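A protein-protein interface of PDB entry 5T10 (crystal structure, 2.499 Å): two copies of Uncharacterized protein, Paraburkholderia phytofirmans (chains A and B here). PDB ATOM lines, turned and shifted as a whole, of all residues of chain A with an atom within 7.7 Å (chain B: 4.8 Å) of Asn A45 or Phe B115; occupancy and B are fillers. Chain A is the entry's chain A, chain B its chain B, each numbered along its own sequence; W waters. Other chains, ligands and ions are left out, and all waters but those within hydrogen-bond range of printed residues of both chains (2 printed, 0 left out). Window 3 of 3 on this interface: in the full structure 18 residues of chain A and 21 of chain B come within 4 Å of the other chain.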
ATOM      1  N   VAL A  23      -5.253  24.833   6.229  1.00  0.00           N
ATOM      2  CA  VAL A  23      -4.307  24.448   7.279  1.00  0.00           C
ATOM      3  C   VAL A  23      -3.058  23.861   6.640  1.00  0.00           C
ATOM      4  O   VAL A  23      -3.143  22.937   5.828  1.00  0.00           O
ATOM      5  CB  VAL A  23      -4.907  23.398   8.244  1.00  0.00           C
ATOM      6  CG1 VAL A  23      -3.886  22.999   9.329  1.00  0.00           C
ATOM      7  CG2 VAL A  23      -6.183  23.921   8.878  1.00  0.00           C
ATOM      8  N   ALA A  39      -2.268  17.744  15.463  1.00  0.00           N
ATOM      9  CA  ALA A  39      -2.628  19.140  15.691  1.00  0.00           C
ATOM     10  C   ALA A  39      -3.299  19.732  14.462  1.00  0.00           C
ATOM     11  O   ALA A  39      -4.240  20.505  14.594  1.00  0.00           O
ATOM     12  CB  ALA A  39      -1.396  19.970  16.101  1.00  0.00           C
ATOM     13  N   GLU A  40      -2.825  19.360  13.270  1.00  0.00           N
ATOM     14  CA  GLU A  40      -3.509  19.753  12.029  1.00  0.00           C
ATOM     15  C   GLU A  40      -4.946  19.249  11.993  1.00  0.00           C
ATOM     16  O   GLU A  40      -5.877  20.011  11.719  1.00  0.00           O
ATOM     17  CB  GLU A  40      -2.770  19.232  10.798  1.00  0.00           C
ATOM     18  CG  GLU A  40      -1.591  20.061  10.392  1.00  0.00           C
ATOM     19  CD  GLU A  40      -0.577  19.281   9.596  1.00  0.00           C
ATOM     20  OE1 GLU A  40      -0.896  18.146   9.193  1.00  0.00           O
ATOM     21  OE2 GLU A  40       0.549  19.795   9.392  1.00  0.00           O
ATOM     22  N   SER A  41      -5.133  17.961  12.265  1.00  0.00           N
ATOM     23  CA  SER A  41      -6.469  17.385  12.163  1.00  0.00           C
ATOM     24  C   SER A  41      -7.409  18.021  13.176  1.00  0.00           C
ATOM     25  O   SER A  41      -8.553  18.292  12.860  1.00  0.00           O
ATOM     26  CB  SER A  41      -6.457  15.852  12.321  1.00  0.00           C
ATOM     27  OG  SER A  41      -5.781  15.220  11.242  1.00  0.00           O
ATOM     28  N   ILE A  42      -6.932  18.263  14.392  1.00  0.00           N
ATOM     29  CA  ILE A  42      -7.803  18.833  15.412  1.00  0.00           C
ATOM     30  C   ILE A  42      -8.135  20.283  15.071  1.00  0.00           C
ATOM     31  O   ILE A  42      -9.264  20.733  15.266  1.00  0.00           O
ATOM     32  CB  ILE A  42      -7.194  18.704  16.808  1.00  0.00           C
ATOM     33  CG1 ILE A  42      -7.209  17.248  17.220  1.00  0.00           C
ATOM     34  CG2 ILE A  42      -7.982  19.483  17.838  1.00  0.00           C
ATOM     35  CD1 ILE A  42      -6.078  16.858  18.172  1.00  0.00           C
ATOM     36  N   ALA A  43      -7.157  20.996  14.529  1.00  0.00           N
ATOM     37  CA  ALA A  43      -7.332  22.400  14.194  1.00  0.00           C
ATOM     38  C   ALA A  43      -8.387  22.545  13.103  1.00  0.00           C
ATOM     39  O   ALA A  43      -9.357  23.297  13.257  1.00  0.00           O
ATOM     40  CB  ALA A  43      -6.016  23.017  13.750  1.00  0.00           C
ATOM     41  N   ALA A  44      -8.192  21.809  12.013  1.00  0.00           N
ATOM     42  CA  ALA A  44      -9.130  21.832  10.903  1.00  0.00           C
ATOM     43  C   ALA A  44     -10.545  21.658  11.418  1.00  0.00           C
ATOM     44  O   ALA A  44     -11.409  22.489  11.126  1.00  0.00           O
ATOM     45  CB  ALA A  44      -8.797  20.753   9.893  1.00  0.00           C
ATOM     46  N   ASN A  45     -10.773  20.612  12.218  1.00  0.00           N
ATOM     47  CA  ASN A  45     -12.107  20.378  12.778  1.00  0.00           C
ATOM     48  C   ASN A  45     -12.600  21.505  13.692  1.00  0.00           C
ATOM     49  O   ASN A  45     -13.803  21.814  13.715  1.00  0.00           O
ATOM     50  CB  ASN A  45     -12.191  19.036  13.498  1.00  0.00           C
ATOM     51  CG  ASN A  45     -12.358  17.879  12.542  1.00  0.00           C
ATOM     52  OD1 ASN A  45     -12.018  17.973  11.364  1.00  0.00           O
ATOM     53  ND2 ASN A  45     -12.882  16.775  13.044  1.00  0.00           N
ATOM     54  N   THR A  46     -11.681  22.119  14.433  1.00  0.00           N
ATOM     55  CA  THR A  46     -12.055  23.207  15.320  1.00  0.00           C
ATOM     56  C   THR A  46     -12.575  24.362  14.476  1.00  0.00           C
ATOM     57  O   THR A  46     -13.596  24.988  14.809  1.00  0.00           O
ATOM     58  CB  THR A  46     -10.863  23.692  16.157  1.00  0.00           C
ATOM     59  OG1 THR A  46     -10.356  22.605  16.935  1.00  0.00           O
ATOM     60  CG2 THR A  46     -11.287  24.790  17.102  1.00  0.00           C
ATOM     61  N   LEU A  47     -11.871  24.626  13.375  1.00  0.00           N
ATOM     62  CA  LEU A  47     -12.240  25.707  12.467  1.00  0.00           C
ATOM     63  C   LEU A  47     -13.593  25.411  11.857  1.00  0.00           C
ATOM     64  O   LEU A  47     -14.458  26.280  11.821  1.00  0.00           O
ATOM     65  CB  LEU A  47     -11.196  25.905  11.364  1.00  0.00           C
ATOM     66  CG  LEU A  47      -9.814  26.443  11.750  1.00  0.00           C
ATOM     67  CD1 LEU A  47      -8.961  26.693  10.506  1.00  0.00           C
ATOM     68  CD2 LEU A  47      -9.892  27.704  12.629  1.00  0.00           C
ATOM     69  N   ARG A  48     -13.788  24.185  11.381  1.00  0.00           N
ATOM     70  CA  ARG A  48     -15.074  23.848  10.796  1.00  0.00           C
ATOM     71  C   ARG A  48     -16.157  23.996  11.854  1.00  0.00           C
ATOM     72  O   ARG A  48     -17.146  24.692  11.621  1.00  0.00           O
ATOM     73  CB  ARG A  48     -15.077  22.469  10.174  1.00  0.00           C
ATOM     74  CG  ARG A  48     -14.168  22.327   8.972  1.00  0.00           C
ATOM     75  CD  ARG A  48     -14.201  20.888   8.450  1.00  0.00           C
ATOM     76  NE  ARG A  48     -13.155  20.659   7.467  1.00  0.00           N
ATOM     77  CZ  ARG A  48     -12.164  19.786   7.627  1.00  0.00           C
ATOM     78  NH1 ARG A  48     -12.109  19.043   8.729  1.00  0.00           N
ATOM     79  NH2 ARG A  48     -11.240  19.643   6.680  1.00  0.00           N
ATOM     80  N   ALA A  49     -15.946  23.416  13.034  1.00  0.00           N
ATOM     81  CA  ALA A  49     -16.924  23.568  14.115  1.00  0.00           C
ATOM     82  C   ALA A  49     -17.171  25.033  14.481  1.00  0.00           C
ATOM     83  O   ALA A  49     -18.227  25.382  14.993  1.00  0.00           O
ATOM     84  CB  ALA A  49     -16.505  22.801  15.328  1.00  0.00           C
ATOM     85  N   GLY A  50     -16.194  25.892  14.222  1.00  0.00           N
ATOM     86  CA  GLY A  50     -16.343  27.295  14.551  1.00  0.00           C
ATOM     87  C   GLY A  50     -17.113  28.031  13.477  1.00  0.00           C
ATOM     88  O   GLY A  50     -17.337  29.232  13.567  1.00  0.00           O
ATOM     89  N   GLY A  51     -17.510  27.304  12.443  1.00  0.00           N
ATOM     90  CA  GLY A  51     -18.380  27.864  11.438  1.00  0.00           C
ATOM     91  C   GLY A  51     -17.694  28.187  10.130  1.00  0.00           C
ATOM     92  O   GLY A  51     -18.361  28.666   9.195  1.00  0.00           O
ATOM     93  N   ILE A  52     -16.384  27.955  10.046  1.00  0.00           N
ATOM     94  CA  ILE A  52     -15.710  28.121   8.761  1.00  0.00           C
ATOM     95  C   ILE A  52     -16.140  26.958   7.892  1.00  0.00           C
ATOM     96  O   ILE A  52     -15.858  25.801   8.201  1.00  0.00           O
ATOM     97  CB  ILE A  52     -14.172  28.152   8.864  1.00  0.00           C
ATOM     98  CG1 ILE A  52     -13.715  29.125   9.956  1.00  0.00           C
ATOM     99  CG2 ILE A  52     -13.548  28.491   7.504  1.00  0.00           C
ATOM    100  CD1 ILE A  52     -14.228  30.508   9.783  1.00  0.00           C
ATOM    101  N   VAL A  55     -12.625  24.425   4.992  1.00  0.00           N
ATOM    102  CA  VAL A  55     -11.299  24.322   5.570  1.00  0.00           C
ATOM    103  C   VAL A  55     -10.663  23.108   4.930  1.00  0.00           C
ATOM    104  O   VAL A  55     -11.256  22.036   4.929  1.00  0.00           O
ATOM    105  CB  VAL A  55     -11.383  24.049   7.067  1.00  0.00           C
ATOM    106  CG1 VAL A  55     -10.003  23.749   7.620  1.00  0.00           C
ATOM    107  CG2 VAL A  55     -12.029  25.218   7.788  1.00  0.00           C
ATOM    108  N   ILE A  57      -6.820  20.839   4.441  1.00  0.00           N
ATOM    109  CA  ILE A  57      -5.485  20.608   4.979  1.00  0.00           C
ATOM    110  C   ILE A  57      -4.524  20.219   3.867  1.00  0.00           C
ATOM    111  O   ILE A  57      -4.773  19.277   3.128  1.00  0.00           O
ATOM    112  CB  ILE A  57      -5.486  19.466   6.005  1.00  0.00           C
ATOM    113  CG1 ILE A  57      -6.429  19.778   7.170  1.00  0.00           C
ATOM    114  CG2 ILE A  57      -4.065  19.181   6.505  1.00  0.00           C
ATOM    115  CD1 ILE A  57      -6.338  18.756   8.285  1.00  0.00           C
ATOM    116  N   ILE A 149      -6.669  23.413  21.934  1.00  0.00           N
ATOM    117  CA  ILE A 149      -6.754  23.892  20.555  1.00  0.00           C
ATOM    118  C   ILE A 149      -8.110  24.553  20.258  1.00  0.00           C
ATOM    119  O   ILE A 149      -8.193  25.501  19.471  1.00  0.00           O
ATOM    120  CB  ILE A 149      -6.438  22.764  19.555  1.00  0.00           C
ATOM    121  CG1 ILE A 149      -4.932  22.508  19.534  1.00  0.00           C
ATOM    122  CG2 ILE A 149      -6.906  23.112  18.155  1.00  0.00           C
ATOM    123  CD1 ILE A 149      -4.518  21.217  18.860  1.00  0.00           C
ATOM    124  N   LEU A 153      -8.103  28.697  19.253  1.00  0.00           N
ATOM    125  CA  LEU A 153      -8.637  29.062  17.941  1.00  0.00           C
ATOM    126  C   LEU A 153     -10.032  29.663  18.014  1.00  0.00           C
ATOM    127  O   LEU A 153     -10.614  30.048  16.990  1.00  0.00           O
ATOM    128  CB  LEU A 153      -8.676  27.843  17.025  1.00  0.00           C
ATOM    129  CG  LEU A 153      -7.324  27.222  16.684  1.00  0.00           C
ATOM    130  CD1 LEU A 153      -7.514  26.097  15.673  1.00  0.00           C
ATOM    131  CD2 LEU A 153      -6.350  28.304  16.182  1.00  0.00           C
ATOM    132  N   ILE B  26      -8.057   5.768   7.337  1.00  0.00           N
ATOM    133  CA  ILE B  26      -8.100   6.568   8.540  1.00  0.00           C
ATOM    134  C   ILE B  26      -6.684   6.583   9.054  1.00  0.00           C
ATOM    135  O   ILE B  26      -6.138   5.546   9.414  1.00  0.00           O
ATOM    136  CB  ILE B  26      -9.081   5.978   9.566  1.00  0.00           C
ATOM    137  CG1 ILE B  26     -10.516   6.375   9.191  1.00  0.00           C
ATOM    138  CG2 ILE B  26      -8.738   6.421  10.978  1.00  0.00           C
ATOM    139  CD1 ILE B  26     -11.581   5.840  10.121  1.00  0.00           C
ATOM    140  N   ALA B  43     -15.739   1.901  12.542  1.00  0.00           N
ATOM    141  CA  ALA B  43     -16.555   2.949  11.920  1.00  0.00           C
ATOM    142  C   ALA B  43     -17.541   2.339  10.927  1.00  0.00           C
ATOM    143  O   ALA B  43     -18.731   2.624  10.986  1.00  0.00           O
ATOM    144  CB  ALA B  43     -15.700   4.012  11.237  1.00  0.00           C
ATOM    145  N   LEU B  92     -16.205   8.623   4.215  1.00  0.00           N
ATOM    146  CA  LEU B  92     -15.886   8.918   5.603  1.00  0.00           C
ATOM    147  C   LEU B  92     -14.418   8.645   5.838  1.00  0.00           C
ATOM    148  O   LEU B  92     -13.951   7.519   5.674  1.00  0.00           O
ATOM    149  CB  LEU B  92     -16.710   8.098   6.596  1.00  0.00           C
ATOM    150  CG  LEU B  92     -16.266   8.373   8.048  1.00  0.00           C
ATOM    151  CD1 LEU B  92     -17.133   9.452   8.696  1.00  0.00           C
ATOM    152  CD2 LEU B  92     -16.257   7.119   8.901  1.00  0.00           C
ATOM    153  N   SER B  93     -13.696   9.685   6.220  1.00  0.00           N
ATOM    154  CA  SER B  93     -12.295   9.540   6.580  1.00  0.00           C
ATOM    155  C   SER B  93     -12.018  10.216   7.909  1.00  0.00           C
ATOM    156  O   SER B  93     -12.899  10.838   8.504  1.00  0.00           O
ATOM    157  CB  SER B  93     -11.395  10.133   5.500  1.00  0.00           C
ATOM    158  OG  SER B  93     -10.037  10.070   5.892  1.00  0.00           O
ATOM    159  N   GLY B  94     -10.781  10.106   8.366  1.00  0.00           N
ATOM    160  CA  GLY B  94     -10.398  10.721   9.616  1.00  0.00           C
ATOM    161  C   GLY B  94      -8.963  10.427   9.969  1.00  0.00           C
ATOM    162  O   GLY B  94      -8.130  10.154   9.100  1.00  0.00           O
ATOM    163  N   VAL B 113     -10.141  10.597  18.323  1.00  0.00           N
ATOM    164  CA  VAL B 113     -10.406  10.454  16.894  1.00  0.00           C
ATOM    165  C   VAL B 113     -10.973  11.726  16.288  1.00  0.00           C
ATOM    166  O   VAL B 113     -11.693  12.477  16.953  1.00  0.00           O
ATOM    167  CB  VAL B 113     -11.370   9.244  16.583  1.00  0.00           C
ATOM    168  CG1 VAL B 113     -10.652   7.908  16.742  1.00  0.00           C
ATOM    169  CG2 VAL B 113     -12.581   9.264  17.473  1.00  0.00           C
ATOM    170  N   THR B 114     -10.616  11.980  15.032  1.00  0.00           N
ATOM    171  CA  THR B 114     -11.326  12.957  14.227  1.00  0.00           C
ATOM    172  C   THR B 114     -11.924  12.284  12.987  1.00  0.00           C
ATOM    173  O   THR B 114     -11.384  11.292  12.484  1.00  0.00           O
ATOM    174  CB  THR B 114     -10.422  14.111  13.787  1.00  0.00           C
ATOM    175  OG1 THR B 114      -9.284  13.586  13.102  1.00  0.00           O
ATOM    176  CG2 THR B 114      -9.976  14.933  14.992  1.00  0.00           C
ATOM    177  N   PHE B 115     -13.035  12.833  12.494  1.00  0.00           N
ATOM    178  CA  PHE B 115     -13.747  12.258  11.349  1.00  0.00           C
ATOM    179  C   PHE B 115     -14.223  13.344  10.377  1.00  0.00           C
ATOM    180  O   PHE B 115     -14.724  14.402  10.799  1.00  0.00           O
ATOM    181  CB  PHE B 115     -14.947  11.430  11.821  1.00  0.00           C
ATOM    182  CG  PHE B 115     -14.599  10.037  12.292  1.00  0.00           C
ATOM    183  CD1 PHE B 115     -14.151   9.069  11.395  1.00  0.00           C
ATOM    184  CD2 PHE B 115     -14.761   9.676  13.622  1.00  0.00           C
ATOM    185  CE1 PHE B 115     -13.848   7.754  11.827  1.00  0.00           C
ATOM    186  CE2 PHE B 115     -14.453   8.364  14.066  1.00  0.00           C
ATOM    187  CZ  PHE B 115     -13.996   7.408  13.162  1.00  0.00           C
ATOM    188  N   GLU B 116     -14.066  13.079   9.079  1.00  0.00           N
ATOM    189  CA  GLU B 116     -14.576  13.965   8.032  1.00  0.00           C
ATOM    190  C   GLU B 116     -15.476  13.177   7.095  1.00  0.00           C
ATOM    191  O   GLU B 116     -15.126  12.077   6.672  1.00  0.00           O
ATOM    192  CB  GLU B 116     -13.436  14.569   7.212  1.00  0.00           C
ATOM    193  CG  GLU B 116     -12.295  15.166   8.037  1.00  0.00           C
ATOM    194  CD  GLU B 116     -11.285  15.910   7.171  1.00  0.00           C
ATOM    195  OE1 GLU B 116     -11.187  15.589   5.965  1.00  0.00           O
ATOM    196  OE2 GLU B 116     -10.597  16.824   7.685  1.00  0.00           O
ATOM    197  N   LEU B 117     -16.642  13.724   6.773  1.00  0.00           N
ATOM    198  CA  LEU B 117     -17.459  13.153   5.722  1.00  0.00           C
ATOM    199  C   LEU B 117     -17.290  13.986   4.465  1.00  0.00           C
ATOM    200  O   LEU B 117     -17.477  15.213   4.484  1.00  0.00           O
ATOM    201  CB  LEU B 117     -18.917  13.110   6.144  1.00  0.00           C
ATOM    202  CG  LEU B 117     -19.840  12.303   5.230  1.00  0.00           C
ATOM    203  CD1 LEU B 117     -19.551  10.791   5.354  1.00  0.00           C
ATOM    204  CD2 LEU B 117     -21.290  12.607   5.530  1.00  0.00           C
ATOM    205  N   TRP B 127     -19.405  17.412   6.802  1.00  0.00           N
ATOM    206  CA  TRP B 127     -19.626  17.098   8.206  1.00  0.00           C
ATOM    207  C   TRP B 127     -18.311  16.681   8.873  1.00  0.00           C
ATOM    208  O   TRP B 127     -17.481  16.021   8.262  1.00  0.00           O
ATOM    209  CB  TRP B 127     -20.697  16.009   8.362  1.00  0.00           C
ATOM    210  CG  TRP B 127     -20.973  15.693   9.790  1.00  0.00           C
ATOM    211  CD1 TRP B 127     -21.861  16.315  10.615  1.00  0.00           C
ATOM    212  CD2 TRP B 127     -20.321  14.690  10.581  1.00  0.00           C
ATOM    213  NE1 TRP B 127     -21.820  15.756  11.866  1.00  0.00           N
ATOM    214  CE2 TRP B 127     -20.874  14.758  11.876  1.00  0.00           C
ATOM    215  CE3 TRP B 127     -19.328  13.740  10.318  1.00  0.00           C
ATOM    216  CZ2 TRP B 127     -20.469  13.905  12.905  1.00  0.00           C
ATOM    217  CZ3 TRP B 127     -18.927  12.893  11.342  1.00  0.00           C
ATOM    218  CH2 TRP B 127     -19.504  12.974  12.612  1.00  0.00           C
ATOM    219  N   SER B 128     -18.120  17.085  10.121  1.00  0.00           N
ATOM    220  CA  SER B 128     -16.889  16.782  10.818  1.00  0.00           C
ATOM    221  C   SER B 128     -17.091  16.699  12.334  1.00  0.00           C
ATOM    222  O   SER B 128     -18.009  17.314  12.898  1.00  0.00           O
ATOM    223  CB  SER B 128     -15.752  17.737  10.417  1.00  0.00           C
ATOM    224  OG  SER B 128     -15.857  19.027  11.011  1.00  0.00           O
ATOM    225  N   ALA B 129     -16.248  15.889  12.975  1.00  0.00           N
ATOM    226  CA  ALA B 129     -16.380  15.609  14.393  1.00  0.00           C
ATOM    227  C   ALA B 129     -15.037  15.290  15.028  1.00  0.00           C
ATOM    228  O   ALA B 129     -14.120  14.776  14.386  1.00  0.00           O
ATOM    229  CB  ALA B 129     -17.360  14.447  14.630  1.00  0.00           C
ATOM    230  N   THR B 130     -14.942  15.588  16.311  1.00  0.00           N
ATOM    231  CA  THR B 130     -13.791  15.201  17.092  1.00  0.00           C
ATOM    232  C   THR B 130     -14.290  14.619  18.399  1.00  0.00           C
ATOM    233  O   THR B 130     -15.205  15.158  19.031  1.00  0.00           O
ATOM    234  CB  THR B 130     -12.870  16.393  17.336  1.00  0.00           C
ATOM    235  OG1 THR B 130     -12.377  16.840  16.070  1.00  0.00           O
ATOM    236  CG2 THR B 130     -11.678  16.003  18.216  1.00  0.00           C
ATOM    237  N   ILE B 149     -16.508   5.887  18.997  1.00  0.00           N
ATOM    238  CA  ILE B 149     -16.750   5.973  17.564  1.00  0.00           C
ATOM    239  C   ILE B 149     -18.259   5.932  17.233  1.00  0.00           C
ATOM    240  O   ILE B 149     -18.725   6.554  16.265  1.00  0.00           O
ATOM    241  CB  ILE B 149     -15.993   4.885  16.805  1.00  0.00           C
ATOM    242  CG1 ILE B 149     -14.494   5.178  16.817  1.00  0.00           C
ATOM    243  CG2 ILE B 149     -16.470   4.796  15.365  1.00  0.00           C
ATOM    244  CD1 ILE B 149     -13.630   3.975  16.438  1.00  0.00           C
ATOM    245  N   VAL B 152     -19.617   9.568  18.361  1.00  0.00           N
ATOM    246  CA  VAL B 152     -19.100  10.488  17.367  1.00  0.00           C
ATOM    247  C   VAL B 152     -19.805  10.364  16.018  1.00  0.00           C
ATOM    248  O   VAL B 152     -20.057  11.366  15.359  1.00  0.00           O
ATOM    249  CB  VAL B 152     -17.575  10.287  17.193  1.00  0.00           C
ATOM    250  CG1 VAL B 152     -17.095  10.753  15.826  1.00  0.00           C
ATOM    251  CG2 VAL B 152     -16.838  10.998  18.299  1.00  0.00           C
ATOM    252  N   LEU B 153     -20.144   9.148  15.610  1.00  0.00           N
ATOM    253  CA  LEU B 153     -20.715   8.952  14.274  1.00  0.00           C
ATOM    254  C   LEU B 153     -22.232   8.965  14.246  1.00  0.00           C
ATOM    255  O   LEU B 153     -22.836   8.749  13.198  1.00  0.00           O
ATOM    256  CB  LEU B 153     -20.202   7.652  13.644  1.00  0.00           C
ATOM    257  CG  LEU B 153     -18.699   7.691  13.375  1.00  0.00           C
ATOM    258  CD1 LEU B 153     -18.241   6.444  12.647  1.00  0.00           C
ATOM    259  CD2 LEU B 153     -18.343   8.983  12.601  1.00  0.00           C
HETATM  260  O   HOH W   1      -8.750  13.974  10.638  1.00  0.00           O
HETATM  261  O   HOH W   2     -15.318  19.428  14.336  1.00  0.00           O
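Of the 19 printed residues of chain A, 3 touch a printed residue of chain B.
Among the printed residues, 8 pairs touch across the chains.
Among the printed residues, Asp or Glu carboxylates within 4 Å of a Lys or Arg side-chain nitrogen of the other chain: Arg A48 with Glu B116 (2.9 Å).
Among the printed residues, pairs that only touch across the chains: Arg A48 with Ser B128 (3.6 Å), Asn A45 with Thr B114 (3.7 Å), Ser A41 with Thr B114 (3.7 Å), Asn A45 with Phe B115 (3.8 Å) and Asn A45 with Ser B128 (3.9 Å).
The guanidinium group (NH1) of Arg A48 is in hydrogen-bond range of the side-chain amide oxygen (OD1) of Asn A45.
The backbone carbonyl oxygen of Val A55 lies within hydrogen-bond range of the guanidinium group of Arg A48 (3.0 Å).
O of Ser B93 is in hydrogen-bond range of N of Glu B116.
O of Ala B129 is in hydrogen-bond range of N of Phe B115 (2.9 Å).
Positions printed for both chains: 43, 149 and 153.
Of the 8 pairs that touch across the chains among the printed residues, none has its exchanged pair printed and touching as well.
Water W1 bridges the side-chain hydroxyl (OG1) of Thr B114 (2.6 Å) and the side-chain hydroxyl (OG) of Ser A41 (3.3 Å).
Water W2 lies within hydrogen-bond range of O of Asn A45 and OG of Ser B128.
O of Ala B129 sits at hydrogen-bond distance from ND2 of Asn A45 (2.7 Å).
The side-chain amide nitrogen of Asn A45 lies within hydrogen-bond range of the side-chain hydroxyl of Thr B130 (3.1 Å).
OE2 of Glu B116 is in salt-bridge range of NH1 of Arg A48, 2.9 Å away.
Printed residues of chain B within 4 Å of Ser A41: Thr B114.
Asn A45 touches just these residues of chain B: Thr B114 (3.7 Å), Phe B115 (3.8 Å), Ser B128 (3.9 Å), Ala B129 (2.7 Å) and Thr B130 (3.1 Å).
Leu B92 touches none of the printed residues of chain A.
Of the printed residues of chain A, Thr B114 touches Ser A41 and Asn A45.
Of chain A, only Asn A45 comes within 4 Å of Phe B115.
Printed residues of chain A within 4 Å of Glu B116: Arg A48 (2.9 Å).
Of the printed residues of chain A, Ser B128 touches Asn A45 (3.9 Å) and Arg A48 (3.6 Å).
Of the printed residues of chain A, Ala B129 touches Asn A45 (2.7 Å).
The nearest residue of chain B that does not touch Asn A45 is Glu B116 (4.1 Å).
The nearest residue of chain A that does not touch Phe B115 is Arg A48 (5.7 Å).
The nearest printed residue of chain A that does not touch Ser B128 is Ala A49 (4.8 Å).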
